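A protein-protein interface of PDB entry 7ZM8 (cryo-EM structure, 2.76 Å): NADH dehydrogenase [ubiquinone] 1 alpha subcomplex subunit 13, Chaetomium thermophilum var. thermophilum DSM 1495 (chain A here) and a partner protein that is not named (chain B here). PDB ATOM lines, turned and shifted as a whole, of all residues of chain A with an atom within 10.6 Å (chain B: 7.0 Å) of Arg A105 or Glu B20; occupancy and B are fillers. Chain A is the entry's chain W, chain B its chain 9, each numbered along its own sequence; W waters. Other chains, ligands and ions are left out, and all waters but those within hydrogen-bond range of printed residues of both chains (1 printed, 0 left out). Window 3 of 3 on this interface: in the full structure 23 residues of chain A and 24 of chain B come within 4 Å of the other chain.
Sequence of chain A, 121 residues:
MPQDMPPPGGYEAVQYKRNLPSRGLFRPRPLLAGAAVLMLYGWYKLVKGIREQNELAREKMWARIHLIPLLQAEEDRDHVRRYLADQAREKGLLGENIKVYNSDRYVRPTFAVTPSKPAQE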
ATOM      1  N   TYR A  83     -19.471  21.198  10.802  1.00  0.00           N
ATOM      2  CA  TYR A  83     -20.698  21.959  11.116  1.00  0.00           C
ATOM      3  C   TYR A  83     -21.161  22.713   9.880  1.00  0.00           C
ATOM      4  O   TYR A  83     -22.345  22.717   9.594  1.00  0.00           O
ATOM      5  CB  TYR A  83     -20.462  22.871  12.316  1.00  0.00           C
ATOM      6  CG  TYR A  83     -21.566  23.867  12.564  1.00  0.00           C
ATOM      7  CD1 TYR A  83     -22.671  23.533  13.326  1.00  0.00           C
ATOM      8  CD2 TYR A  83     -21.521  25.134  12.011  1.00  0.00           C
ATOM      9  CE1 TYR A  83     -23.697  24.434  13.539  1.00  0.00           C
ATOM     10  CE2 TYR A  83     -22.540  26.047  12.212  1.00  0.00           C
ATOM     11  CZ  TYR A  83     -23.630  25.695  12.980  1.00  0.00           C
ATOM     12  OH  TYR A  83     -24.634  26.595  13.183  1.00  0.00           O
ATOM     13  N   GLN A  87     -24.609  22.002   7.850  1.00  0.00           N
ATOM     14  CA  GLN A  87     -25.536  23.130   7.622  1.00  0.00           C
ATOM     15  C   GLN A  87     -25.881  23.207   6.137  1.00  0.00           C
ATOM     16  O   GLN A  87     -27.026  23.543   5.823  1.00  0.00           O
ATOM     17  CB  GLN A  87     -24.935  24.416   8.182  1.00  0.00           C
ATOM     18  CG  GLN A  87     -24.949  24.472   9.701  1.00  0.00           C
ATOM     19  CD  GLN A  87     -26.335  24.318  10.269  1.00  0.00           C
ATOM     20  OE1 GLN A  87     -27.259  25.035   9.899  1.00  0.00           O
ATOM     21  NE2 GLN A  87     -26.487  23.390  11.196  1.00  0.00           N
ATOM     22  N   LYS A  99     -33.432  25.054  13.464  1.00  0.00           N
ATOM     23  CA  LYS A  99     -32.712  25.540  14.633  1.00  0.00           C
ATOM     24  C   LYS A  99     -33.021  24.663  15.839  1.00  0.00           C
ATOM     25  O   LYS A  99     -34.185  24.370  16.123  1.00  0.00           O
ATOM     26  CB  LYS A  99     -33.091  26.990  14.925  1.00  0.00           C
ATOM     27  CG  LYS A  99     -32.153  27.690  15.887  1.00  0.00           C
ATOM     28  CD  LYS A  99     -30.898  28.172  15.178  1.00  0.00           C
ATOM     29  CE  LYS A  99     -29.907  28.775  16.163  1.00  0.00           C
ATOM     30  NZ  LYS A  99     -30.489  29.921  16.917  1.00  0.00           N
ATOM     31  N   VAL A 100     -31.979  24.246  16.547  1.00  0.00           N
ATOM     32  CA  VAL A 100     -32.122  23.352  17.687  1.00  0.00           C
ATOM     33  C   VAL A 100     -32.068  24.115  19.000  1.00  0.00           C
ATOM     34  O   VAL A 100     -32.879  23.882  19.895  1.00  0.00           O
ATOM     35  CB  VAL A 100     -31.046  22.247  17.638  1.00  0.00           C
ATOM     36  CG1 VAL A 100     -31.106  21.409  18.890  1.00  0.00           C
ATOM     37  CG2 VAL A 100     -31.226  21.393  16.403  1.00  0.00           C
ATOM     38  N   TYR A 101     -31.107  25.038  19.088  1.00  0.00           N
ATOM     39  CA  TYR A 101     -30.931  25.860  20.303  1.00  0.00           C
ATOM     40  C   TYR A 101     -31.320  27.295  19.964  1.00  0.00           C
ATOM     41  O   TYR A 101     -30.938  27.749  18.900  1.00  0.00           O
ATOM     42  CB  TYR A 101     -29.490  25.724  20.784  1.00  0.00           C
ATOM     43  CG  TYR A 101     -29.134  24.401  21.407  1.00  0.00           C
ATOM     44  CD1 TYR A 101     -29.309  24.186  22.762  1.00  0.00           C
ATOM     45  CD2 TYR A 101     -28.609  23.369  20.646  1.00  0.00           C
ATOM     46  CE1 TYR A 101     -28.977  22.979  23.349  1.00  0.00           C
ATOM     47  CE2 TYR A 101     -28.280  22.152  21.217  1.00  0.00           C
ATOM     48  CZ  TYR A 101     -28.459  21.961  22.573  1.00  0.00           C
ATOM     49  OH  TYR A 101     -28.131  20.770  23.144  1.00  0.00           O
ATOM     50  N   ASN A 102     -32.036  27.986  20.844  1.00  0.00           N
ATOM     51  CA  ASN A 102     -32.468  29.389  20.621  1.00  0.00           C
ATOM     52  C   ASN A 102     -31.249  30.300  20.741  1.00  0.00           C
ATOM     53  O   ASN A 102     -31.302  31.408  20.195  1.00  0.00           O
ATOM     54  CB  ASN A 102     -33.558  29.757  21.623  1.00  0.00           C
ATOM     55  CG  ASN A 102     -34.700  28.766  21.677  1.00  0.00           C
ATOM     56  OD1 ASN A 102     -35.441  28.614  20.714  1.00  0.00           O
ATOM     57  ND2 ASN A 102     -34.864  28.101  22.807  1.00  0.00           N
ATOM     58  N   SER A 103     -30.189  29.839  21.394  1.00  0.00           N
ATOM     59  CA  SER A 103     -28.913  30.589  21.501  1.00  0.00           C
ATOM     60  C   SER A 103     -28.042  30.361  20.264  1.00  0.00           C
ATOM     61  O   SER A 103     -28.273  29.377  19.550  1.00  0.00           O
ATOM     62  CB  SER A 103     -28.165  30.214  22.734  1.00  0.00           C
ATOM     63  OG  SER A 103     -27.935  28.814  22.783  1.00  0.00           O
ATOM     64  N   ASP A 104     -27.037  31.216  20.061  1.00  0.00           N
ATOM     65  CA  ASP A 104     -26.142  31.118  18.876  1.00  0.00           C
ATOM     66  C   ASP A 104     -24.880  30.331  19.225  1.00  0.00           C
ATOM     67  O   ASP A 104     -24.000  30.280  18.376  1.00  0.00           O
ATOM     68  CB  ASP A 104     -25.784  32.499  18.325  1.00  0.00           C
ATOM     69  CG  ASP A 104     -24.897  33.323  19.243  1.00  0.00           C
ATOM     70  OD1 ASP A 104     -25.110  33.271  20.470  1.00  0.00           O
ATOM     71  OD2 ASP A 104     -23.991  34.003  18.721  1.00  0.00           O
ATOM     72  N   ARG A 105     -24.830  29.709  20.401  1.00  0.00           N
ATOM     73  CA  ARG A 105     -23.643  28.942  20.864  1.00  0.00           C
ATOM     74  C   ARG A 105     -23.383  27.731  19.980  1.00  0.00           C
ATOM     75  O   ARG A 105     -24.343  27.193  19.428  1.00  0.00           O
ATOM     76  CB  ARG A 105     -23.862  28.397  22.280  1.00  0.00           C
ATOM     77  CG  ARG A 105     -23.548  29.390  23.387  1.00  0.00           C
ATOM     78  CD  ARG A 105     -24.078  28.931  24.731  1.00  0.00           C
ATOM     79  NE  ARG A 105     -23.644  27.594  25.110  1.00  0.00           N
ATOM     80  CZ  ARG A 105     -22.550  27.324  25.810  1.00  0.00           C
ATOM     81  NH1 ARG A 105     -21.753  28.299  26.204  1.00  0.00           N
ATOM     82  NH2 ARG A 105     -22.254  26.076  26.112  1.00  0.00           N
ATOM     83  N   TYR A 106     -22.118  27.328  19.851  1.00  0.00           N
ATOM     84  CA  TYR A 106     -21.825  26.071  19.123  1.00  0.00           C
ATOM     85  C   TYR A 106     -21.945  24.938  20.123  1.00  0.00           C
ATOM     86  O   TYR A 106     -21.203  24.897  21.104  1.00  0.00           O
ATOM     87  CB  TYR A 106     -20.438  26.046  18.479  1.00  0.00           C
ATOM     88  CG  TYR A 106     -20.017  24.676  18.016  1.00  0.00           C
ATOM     89  CD1 TYR A 106     -20.703  24.022  17.009  1.00  0.00           C
ATOM     90  CD2 TYR A 106     -18.949  24.023  18.605  1.00  0.00           C
ATOM     91  CE1 TYR A 106     -20.338  22.755  16.594  1.00  0.00           C
ATOM     92  CE2 TYR A 106     -18.570  22.757  18.202  1.00  0.00           C
ATOM     93  CZ  TYR A 106     -19.265  22.124  17.191  1.00  0.00           C
ATOM     94  OH  TYR A 106     -18.891  20.876  16.792  1.00  0.00           O
ATOM     95  N   VAL A 107     -22.862  24.027  19.844  1.00  0.00           N
ATOM     96  CA  VAL A 107     -23.017  22.838  20.718  1.00  0.00           C
ATOM     97  C   VAL A 107     -22.451  21.662  19.921  1.00  0.00           C
ATOM     98  O   VAL A 107     -22.825  21.527  18.761  1.00  0.00           O
ATOM     99  CB  VAL A 107     -24.476  22.659  21.196  1.00  0.00           C
ATOM    100  CG1 VAL A 107     -24.552  21.701  22.369  1.00  0.00           C
ATOM    101  CG2 VAL A 107     -25.103  23.990  21.569  1.00  0.00           C
ATOM    102  N   ARG A 108     -21.534  20.897  20.508  1.00  0.00           N
ATOM    103  CA  ARG A 108     -20.867  19.766  19.810  1.00  0.00           C
ATOM    104  C   ARG A 108     -21.902  18.685  19.505  1.00  0.00           C
ATOM    105  O   ARG A 108     -22.598  18.297  20.456  1.00  0.00           O
ATOM    106  CB  ARG A 108     -19.649  19.265  20.591  1.00  0.00           C
ATOM    107  CG  ARG A 108     -18.510  20.265  20.707  1.00  0.00           C
ATOM    108  CD  ARG A 108     -17.602  19.907  21.863  1.00  0.00           C
ATOM    109  NE  ARG A 108     -16.794  18.730  21.602  1.00  0.00           N
ATOM    110  CZ  ARG A 108     -15.527  18.760  21.211  1.00  0.00           C
ATOM    111  NH1 ARG A 108     -14.876  17.630  20.994  1.00  0.00           N
ATOM    112  NH2 ARG A 108     -14.919  19.918  21.030  1.00  0.00           N
ATOM    113  N   PRO A 109     -22.032  18.158  18.254  1.00  0.00           N
ATOM    114  CA  PRO A 109     -23.128  17.240  17.956  1.00  0.00           C
ATOM    115  C   PRO A 109     -23.297  15.962  18.796  1.00  0.00           C
ATOM    116  O   PRO A 109     -22.337  15.378  19.153  1.00  0.00           O
ATOM    117  CB  PRO A 109     -22.849  16.954  16.481  1.00  0.00           C
ATOM    118  CG  PRO A 109     -21.407  17.254  16.251  1.00  0.00           C
ATOM    119  CD  PRO A 109     -21.169  18.456  17.120  1.00  0.00           C
ATOM    120  N   ARG B  13     -21.288  18.965  31.202  1.00  0.00           N
ATOM    121  CA  ARG B  13     -21.583  19.492  29.837  1.00  0.00           C
ATOM    122  C   ARG B  13     -22.706  20.522  29.804  1.00  0.00           C
ATOM    123  O   ARG B  13     -22.614  21.435  28.984  1.00  0.00           O
ATOM    124  CB  ARG B  13     -21.844  18.358  28.839  1.00  0.00           C
ATOM    125  CG  ARG B  13     -22.901  17.354  29.259  1.00  0.00           C
ATOM    126  CD  ARG B  13     -23.107  16.360  28.138  1.00  0.00           C
ATOM    127  NE  ARG B  13     -24.337  15.635  28.385  1.00  0.00           N
ATOM    128  CZ  ARG B  13     -25.514  16.022  27.931  1.00  0.00           C
ATOM    129  NH1 ARG B  13     -26.596  15.322  28.213  1.00  0.00           N
ATOM    130  NH2 ARG B  13     -25.602  17.112  27.196  1.00  0.00           N
ATOM    131  N   PHE B  15     -23.738  22.416  32.347  1.00  0.00           N
ATOM    132  CA  PHE B  15     -23.563  23.486  33.361  1.00  0.00           C
ATOM    133  C   PHE B  15     -23.573  24.886  32.725  1.00  0.00           C
ATOM    134  O   PHE B  15     -24.159  25.778  33.341  1.00  0.00           O
ATOM    135  CB  PHE B  15     -22.365  23.188  34.259  1.00  0.00           C
ATOM    136  CG  PHE B  15     -22.188  24.125  35.423  1.00  0.00           C
ATOM    137  CD1 PHE B  15     -23.104  24.143  36.460  1.00  0.00           C
ATOM    138  CD2 PHE B  15     -21.096  24.972  35.490  1.00  0.00           C
ATOM    139  CE1 PHE B  15     -22.932  24.991  37.539  1.00  0.00           C
ATOM    140  CE2 PHE B  15     -20.929  25.821  36.571  1.00  0.00           C
ATOM    141  CZ  PHE B  15     -21.843  25.823  37.595  1.00  0.00           C
ATOM    142  N   PRO B  16     -22.993  25.154  31.534  1.00  0.00           N
ATOM    143  CA  PRO B  16     -23.071  26.495  30.964  1.00  0.00           C
ATOM    144  C   PRO B  16     -24.506  26.997  30.731  1.00  0.00           C
ATOM    145  O   PRO B  16     -24.772  28.109  31.086  1.00  0.00           O
ATOM    146  CB  PRO B  16     -22.348  26.318  29.630  1.00  0.00           C
ATOM    147  CG  PRO B  16     -21.337  25.262  29.902  1.00  0.00           C
ATOM    148  CD  PRO B  16     -22.106  24.286  30.756  1.00  0.00           C
ATOM    149  N   PHE B  17     -25.396  26.152  30.229  1.00  0.00           N
ATOM    150  CA  PHE B  17     -26.820  26.491  29.999  1.00  0.00           C
ATOM    151  C   PHE B  17     -27.544  26.796  31.309  1.00  0.00           C
ATOM    152  O   PHE B  17     -28.391  27.681  31.287  1.00  0.00           O
ATOM    153  CB  PHE B  17     -27.467  25.329  29.238  1.00  0.00           C
ATOM    154  CG  PHE B  17     -26.951  25.123  27.836  1.00  0.00           C
ATOM    155  CD1 PHE B  17     -25.831  24.343  27.596  1.00  0.00           C
ATOM    156  CD2 PHE B  17     -27.581  25.722  26.760  1.00  0.00           C
ATOM    157  CE1 PHE B  17     -25.359  24.161  26.306  1.00  0.00           C
ATOM    158  CE2 PHE B  17     -27.105  25.540  25.472  1.00  0.00           C
ATOM    159  CZ  PHE B  17     -26.000  24.756  25.247  1.00  0.00           C
ATOM    160  N   TRP B  18     -27.275  26.044  32.368  1.00  0.00           N
ATOM    161  CA  TRP B  18     -27.889  26.244  33.706  1.00  0.00           C
ATOM    162  C   TRP B  18     -27.493  27.597  34.294  1.00  0.00           C
ATOM    163  O   TRP B  18     -28.350  28.248  34.862  1.00  0.00           O
ATOM    164  CB  TRP B  18     -27.428  25.101  34.621  1.00  0.00           C
ATOM    165  CG  TRP B  18     -27.994  25.155  36.004  1.00  0.00           C
ATOM    166  CD1 TRP B  18     -27.321  25.405  37.163  1.00  0.00           C
ATOM    167  CD2 TRP B  18     -29.369  24.964  36.371  1.00  0.00           C
ATOM    168  NE1 TRP B  18     -28.179  25.373  38.227  1.00  0.00           N
ATOM    169  CE2 TRP B  18     -29.441  25.097  37.773  1.00  0.00           C
ATOM    170  CE3 TRP B  18     -30.539  24.694  35.657  1.00  0.00           C
ATOM    171  CZ2 TRP B  18     -30.643  24.978  38.466  1.00  0.00           C
ATOM    172  CZ3 TRP B  18     -31.722  24.566  36.344  1.00  0.00           C
ATOM    173  CH2 TRP B  18     -31.771  24.703  37.729  1.00  0.00           C
ATOM    174  N   GLN B  19     -26.222  27.971  34.177  1.00  0.00           N
ATOM    175  CA  GLN B  19     -25.733  29.274  34.685  1.00  0.00           C
ATOM    176  C   GLN B  19     -26.322  30.378  33.813  1.00  0.00           C
ATOM    177  O   GLN B  19     -26.610  31.441  34.357  1.00  0.00           O
ATOM    178  CB  GLN B  19     -24.211  29.287  34.643  1.00  0.00           C
ATOM    179  CG  GLN B  19     -23.583  28.320  35.628  1.00  0.00           C
ATOM    180  CD  GLN B  19     -22.625  29.023  36.554  1.00  0.00           C
ATOM    181  OE1 GLN B  19     -22.870  29.151  37.749  1.00  0.00           O
ATOM    182  NE2 GLN B  19     -21.519  29.489  35.999  1.00  0.00           N
ATOM    183  N   GLU B  20     -26.479  30.128  32.517  1.00  0.00           N
ATOM    184  CA  GLU B  20     -27.123  31.092  31.594  1.00  0.00           C
ATOM    185  C   GLU B  20     -28.592  31.232  31.964  1.00  0.00           C
ATOM    186  O   GLU B  20     -29.145  32.302  31.723  1.00  0.00           O
ATOM    187  CB  GLU B  20     -26.940  30.645  30.145  1.00  0.00           C
ATOM    188  CG  GLU B  20     -25.560  30.937  29.592  1.00  0.00           C
ATOM    189  CD  GLU B  20     -25.312  30.421  28.186  1.00  0.00           C
ATOM    190  OE1 GLU B  20     -24.793  31.201  27.361  1.00  0.00           O
ATOM    191  OE2 GLU B  20     -25.622  29.240  27.921  1.00  0.00           O
ATOM    192  N   LEU B  21     -29.204  30.177  32.495  1.00  0.00           N
ATOM    193  CA  LEU B  21     -30.636  30.211  32.872  1.00  0.00           C
ATOM    194  C   LEU B  21     -30.777  30.932  34.208  1.00  0.00           C
ATOM    195  O   LEU B  21     -31.695  31.756  34.333  1.00  0.00           O
ATOM    196  CB  LEU B  21     -31.155  28.775  32.964  1.00  0.00           C
ATOM    197  CG  LEU B  21     -32.621  28.621  33.366  1.00  0.00           C
ATOM    198  CD1 LEU B  21     -33.525  29.426  32.447  1.00  0.00           C
ATOM    199  CD2 LEU B  21     -33.025  27.158  33.367  1.00  0.00           C
ATOM    200  N   LEU B  22     -29.911  30.611  35.168  1.00  0.00           N
ATOM    201  CA  LEU B  22     -29.948  31.250  36.506  1.00  0.00           C
ATOM    202  C   LEU B  22     -29.627  32.731  36.355  1.00  0.00           C
ATOM    203  O   LEU B  22     -30.264  33.537  37.040  1.00  0.00           O
ATOM    204  CB  LEU B  22     -28.935  30.556  37.419  1.00  0.00           C
ATOM    205  CG  LEU B  22     -29.331  29.175  37.934  1.00  0.00           C
ATOM    206  CD1 LEU B  22     -28.358  28.717  39.005  1.00  0.00           C
ATOM    207  CD2 LEU B  22     -30.747  29.188  38.480  1.00  0.00           C
ATOM    208  N   ALA B  23     -28.657  33.051  35.504  1.00  0.00           N
ATOM    209  CA  ALA B  23     -28.312  34.464  35.248  1.00  0.00           C
ATOM    210  C   ALA B  23     -29.548  35.179  34.704  1.00  0.00           C
ATOM    211  O   ALA B  23     -29.925  36.204  35.282  1.00  0.00           O
ATOM    212  CB  ALA B  23     -27.151  34.565  34.304  1.00  0.00           C
ATOM    213  N   CYS B  24     -30.172  34.621  33.664  1.00  0.00           N
ATOM    214  CA  CYS B  24     -31.373  35.273  33.102  1.00  0.00           C
ATOM    215  C   CYS B  24     -32.429  35.522  34.184  1.00  0.00           C
ATOM    216  O   CYS B  24     -32.830  36.678  34.313  1.00  0.00           O
ATOM    217  CB  CYS B  24     -31.927  34.455  31.944  1.00  0.00           C
ATOM    218  SG  CYS B  24     -33.024  35.390  30.852  1.00  0.00           S
ATOM    219  N   TYR B  25     -32.831  34.503  34.946  1.00  0.00           N
ATOM    220  CA  TYR B  25     -33.911  34.664  35.955  1.00  0.00           C
ATOM    221  C   TYR B  25     -33.568  35.743  36.982  1.00  0.00           C
ATOM    222  O   TYR B  25     -34.400  36.628  37.207  1.00  0.00           O
ATOM    223  CB  TYR B  25     -34.177  33.345  36.677  1.00  0.00           C
ATOM    224  CG  TYR B  25     -35.401  33.333  37.557  1.00  0.00           C
ATOM    225  CD1 TYR B  25     -36.659  33.110  37.026  1.00  0.00           C
ATOM    226  CD2 TYR B  25     -35.303  33.535  38.924  1.00  0.00           C
ATOM    227  CE1 TYR B  25     -37.788  33.092  37.826  1.00  0.00           C
ATOM    228  CE2 TYR B  25     -36.422  33.523  39.738  1.00  0.00           C
ATOM    229  CZ  TYR B  25     -37.670  33.302  39.187  1.00  0.00           C
ATOM    230  OH  TYR B  25     -38.778  33.287  39.982  1.00  0.00           O
ATOM    231  N   CYS B  40     -36.832  34.094  30.106  1.00  0.00           N
ATOM    232  CA  CYS B  40     -36.190  32.845  30.486  1.00  0.00           C
ATOM    233  C   CYS B  40     -36.742  31.633  29.752  1.00  0.00           C
ATOM    234  O   CYS B  40     -36.161  30.553  29.865  1.00  0.00           O
ATOM    235  CB  CYS B  40     -36.358  32.622  31.987  1.00  0.00           C
ATOM    236  SG  CYS B  40     -35.535  33.812  33.016  1.00  0.00           S
ATOM    237  N   VAL B  43     -34.291  30.173  27.167  1.00  0.00           N
ATOM    238  CA  VAL B  43     -33.056  29.723  27.856  1.00  0.00           C
ATOM    239  C   VAL B  43     -33.300  28.391  28.581  1.00  0.00           C
ATOM    240  O   VAL B  43     -32.395  27.546  28.577  1.00  0.00           O
ATOM    241  CB  VAL B  43     -32.517  30.862  28.750  1.00  0.00           C
ATOM    242  CG1 VAL B  43     -31.067  30.658  29.146  1.00  0.00           C
ATOM    243  CG2 VAL B  43     -32.695  32.215  28.088  1.00  0.00           C
ATOM    244  N   ASP B  46     -33.317  25.525  26.062  1.00  0.00           N
ATOM    245  CA  ASP B  46     -31.929  25.209  25.662  1.00  0.00           C
ATOM    246  C   ASP B  46     -31.271  24.308  26.701  1.00  0.00           C
ATOM    247  O   ASP B  46     -30.444  23.486  26.321  1.00  0.00           O
ATOM    248  CB  ASP B  46     -31.169  26.485  25.336  1.00  0.00           C
ATOM    249  CG  ASP B  46     -31.457  27.043  23.961  1.00  0.00           C
ATOM    250  OD1 ASP B  46     -32.458  26.632  23.366  1.00  0.00           O
ATOM    251  OD2 ASP B  46     -30.661  27.869  23.495  1.00  0.00           O
HETATM  252  O   HOH W   1     -33.804  24.745  22.108  1.00  0.00           O
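The side-chain carboxylate (OD1) of Asp B46 sits at hydrogen-bond distance from the side-chain amide nitrogen (ND2) of Asn A102, at 2.9 Å.
OD2 of Asp B46 is in hydrogen-bond range of N of Ser A103, 2.9 Å away.
OE2 of Glu B20 lies within salt-bridge range of NE of Arg A105 (3.8 Å).
The side-chain amino group (NZ) of Lys A99 sits at hydrogen-bond distance from the backbone carbonyl oxygen (O) of Tyr A101 (3.0 Å).
NZ of Lys A99 lies within hydrogen-bond range of O of Ser A103 (3.5 Å).
Phe B17 touches Tyr A101 (CE2 to CD1, 3.7 Å).
Asp B46 touches Tyr A101 (O to CE1, 3.4 Å).
Pro B16 touches Arg A105 (CB to NH2, 3.5 Å).
Arg A105 touches Phe B17 (NH2 to CE1, 3.7 Å).
Val A107 touches Phe B17.
Printed residues of chain B within 4 Å of Asn A102: Asp B46.
Of the printed residues of chain B, Ser A103 touches Asp B46.
Arg A105 touches just these residues of chain B: Pro B16, Phe B17 and Glu B20.
Of chain A, only Arg A105 (3.5 Å) comes within 4 Å of Pro B16.
Glu B20 touches one residue of chain A.
No residue of chain A comes within 4 Å of Leu B21.
No residue of chain A comes within 4 Å of Cys B24.
Printed residues of chain A within 4 Å of Asp B46: Tyr A101, Asn A102 and Ser A103.
The nearest printed residue of chain B that does not touch Tyr A101 is Arg B13 (6.0 Å).
Printed residues of chain A that touch a printed residue of chain B: Tyr A101, Asn A102, Ser A103, Arg A105 and Val A107.
Of the 15 printed residues of chain B, 4 touch a printed residue of chain A.
Printed residues of chain B that touch a printed residue of chain A: Pro B16, Phe B17, Glu B20 and Asp B46.
Hydrophobic or aromatic side chains of chain B that line the printed part of chain A: Pro B16 and Phe B17.
Along chain B the printed residues that touch a printed residue of chain A span positions 16 to 46.
Among the printed residues, 8 pairs touch across the chains.
Water W1 lies within hydrogen-bond range of the backbone carbonyl oxygen of Val A100 (2.5 Å) and the side-chain carboxylate of Asp B46 (2.6 Å).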
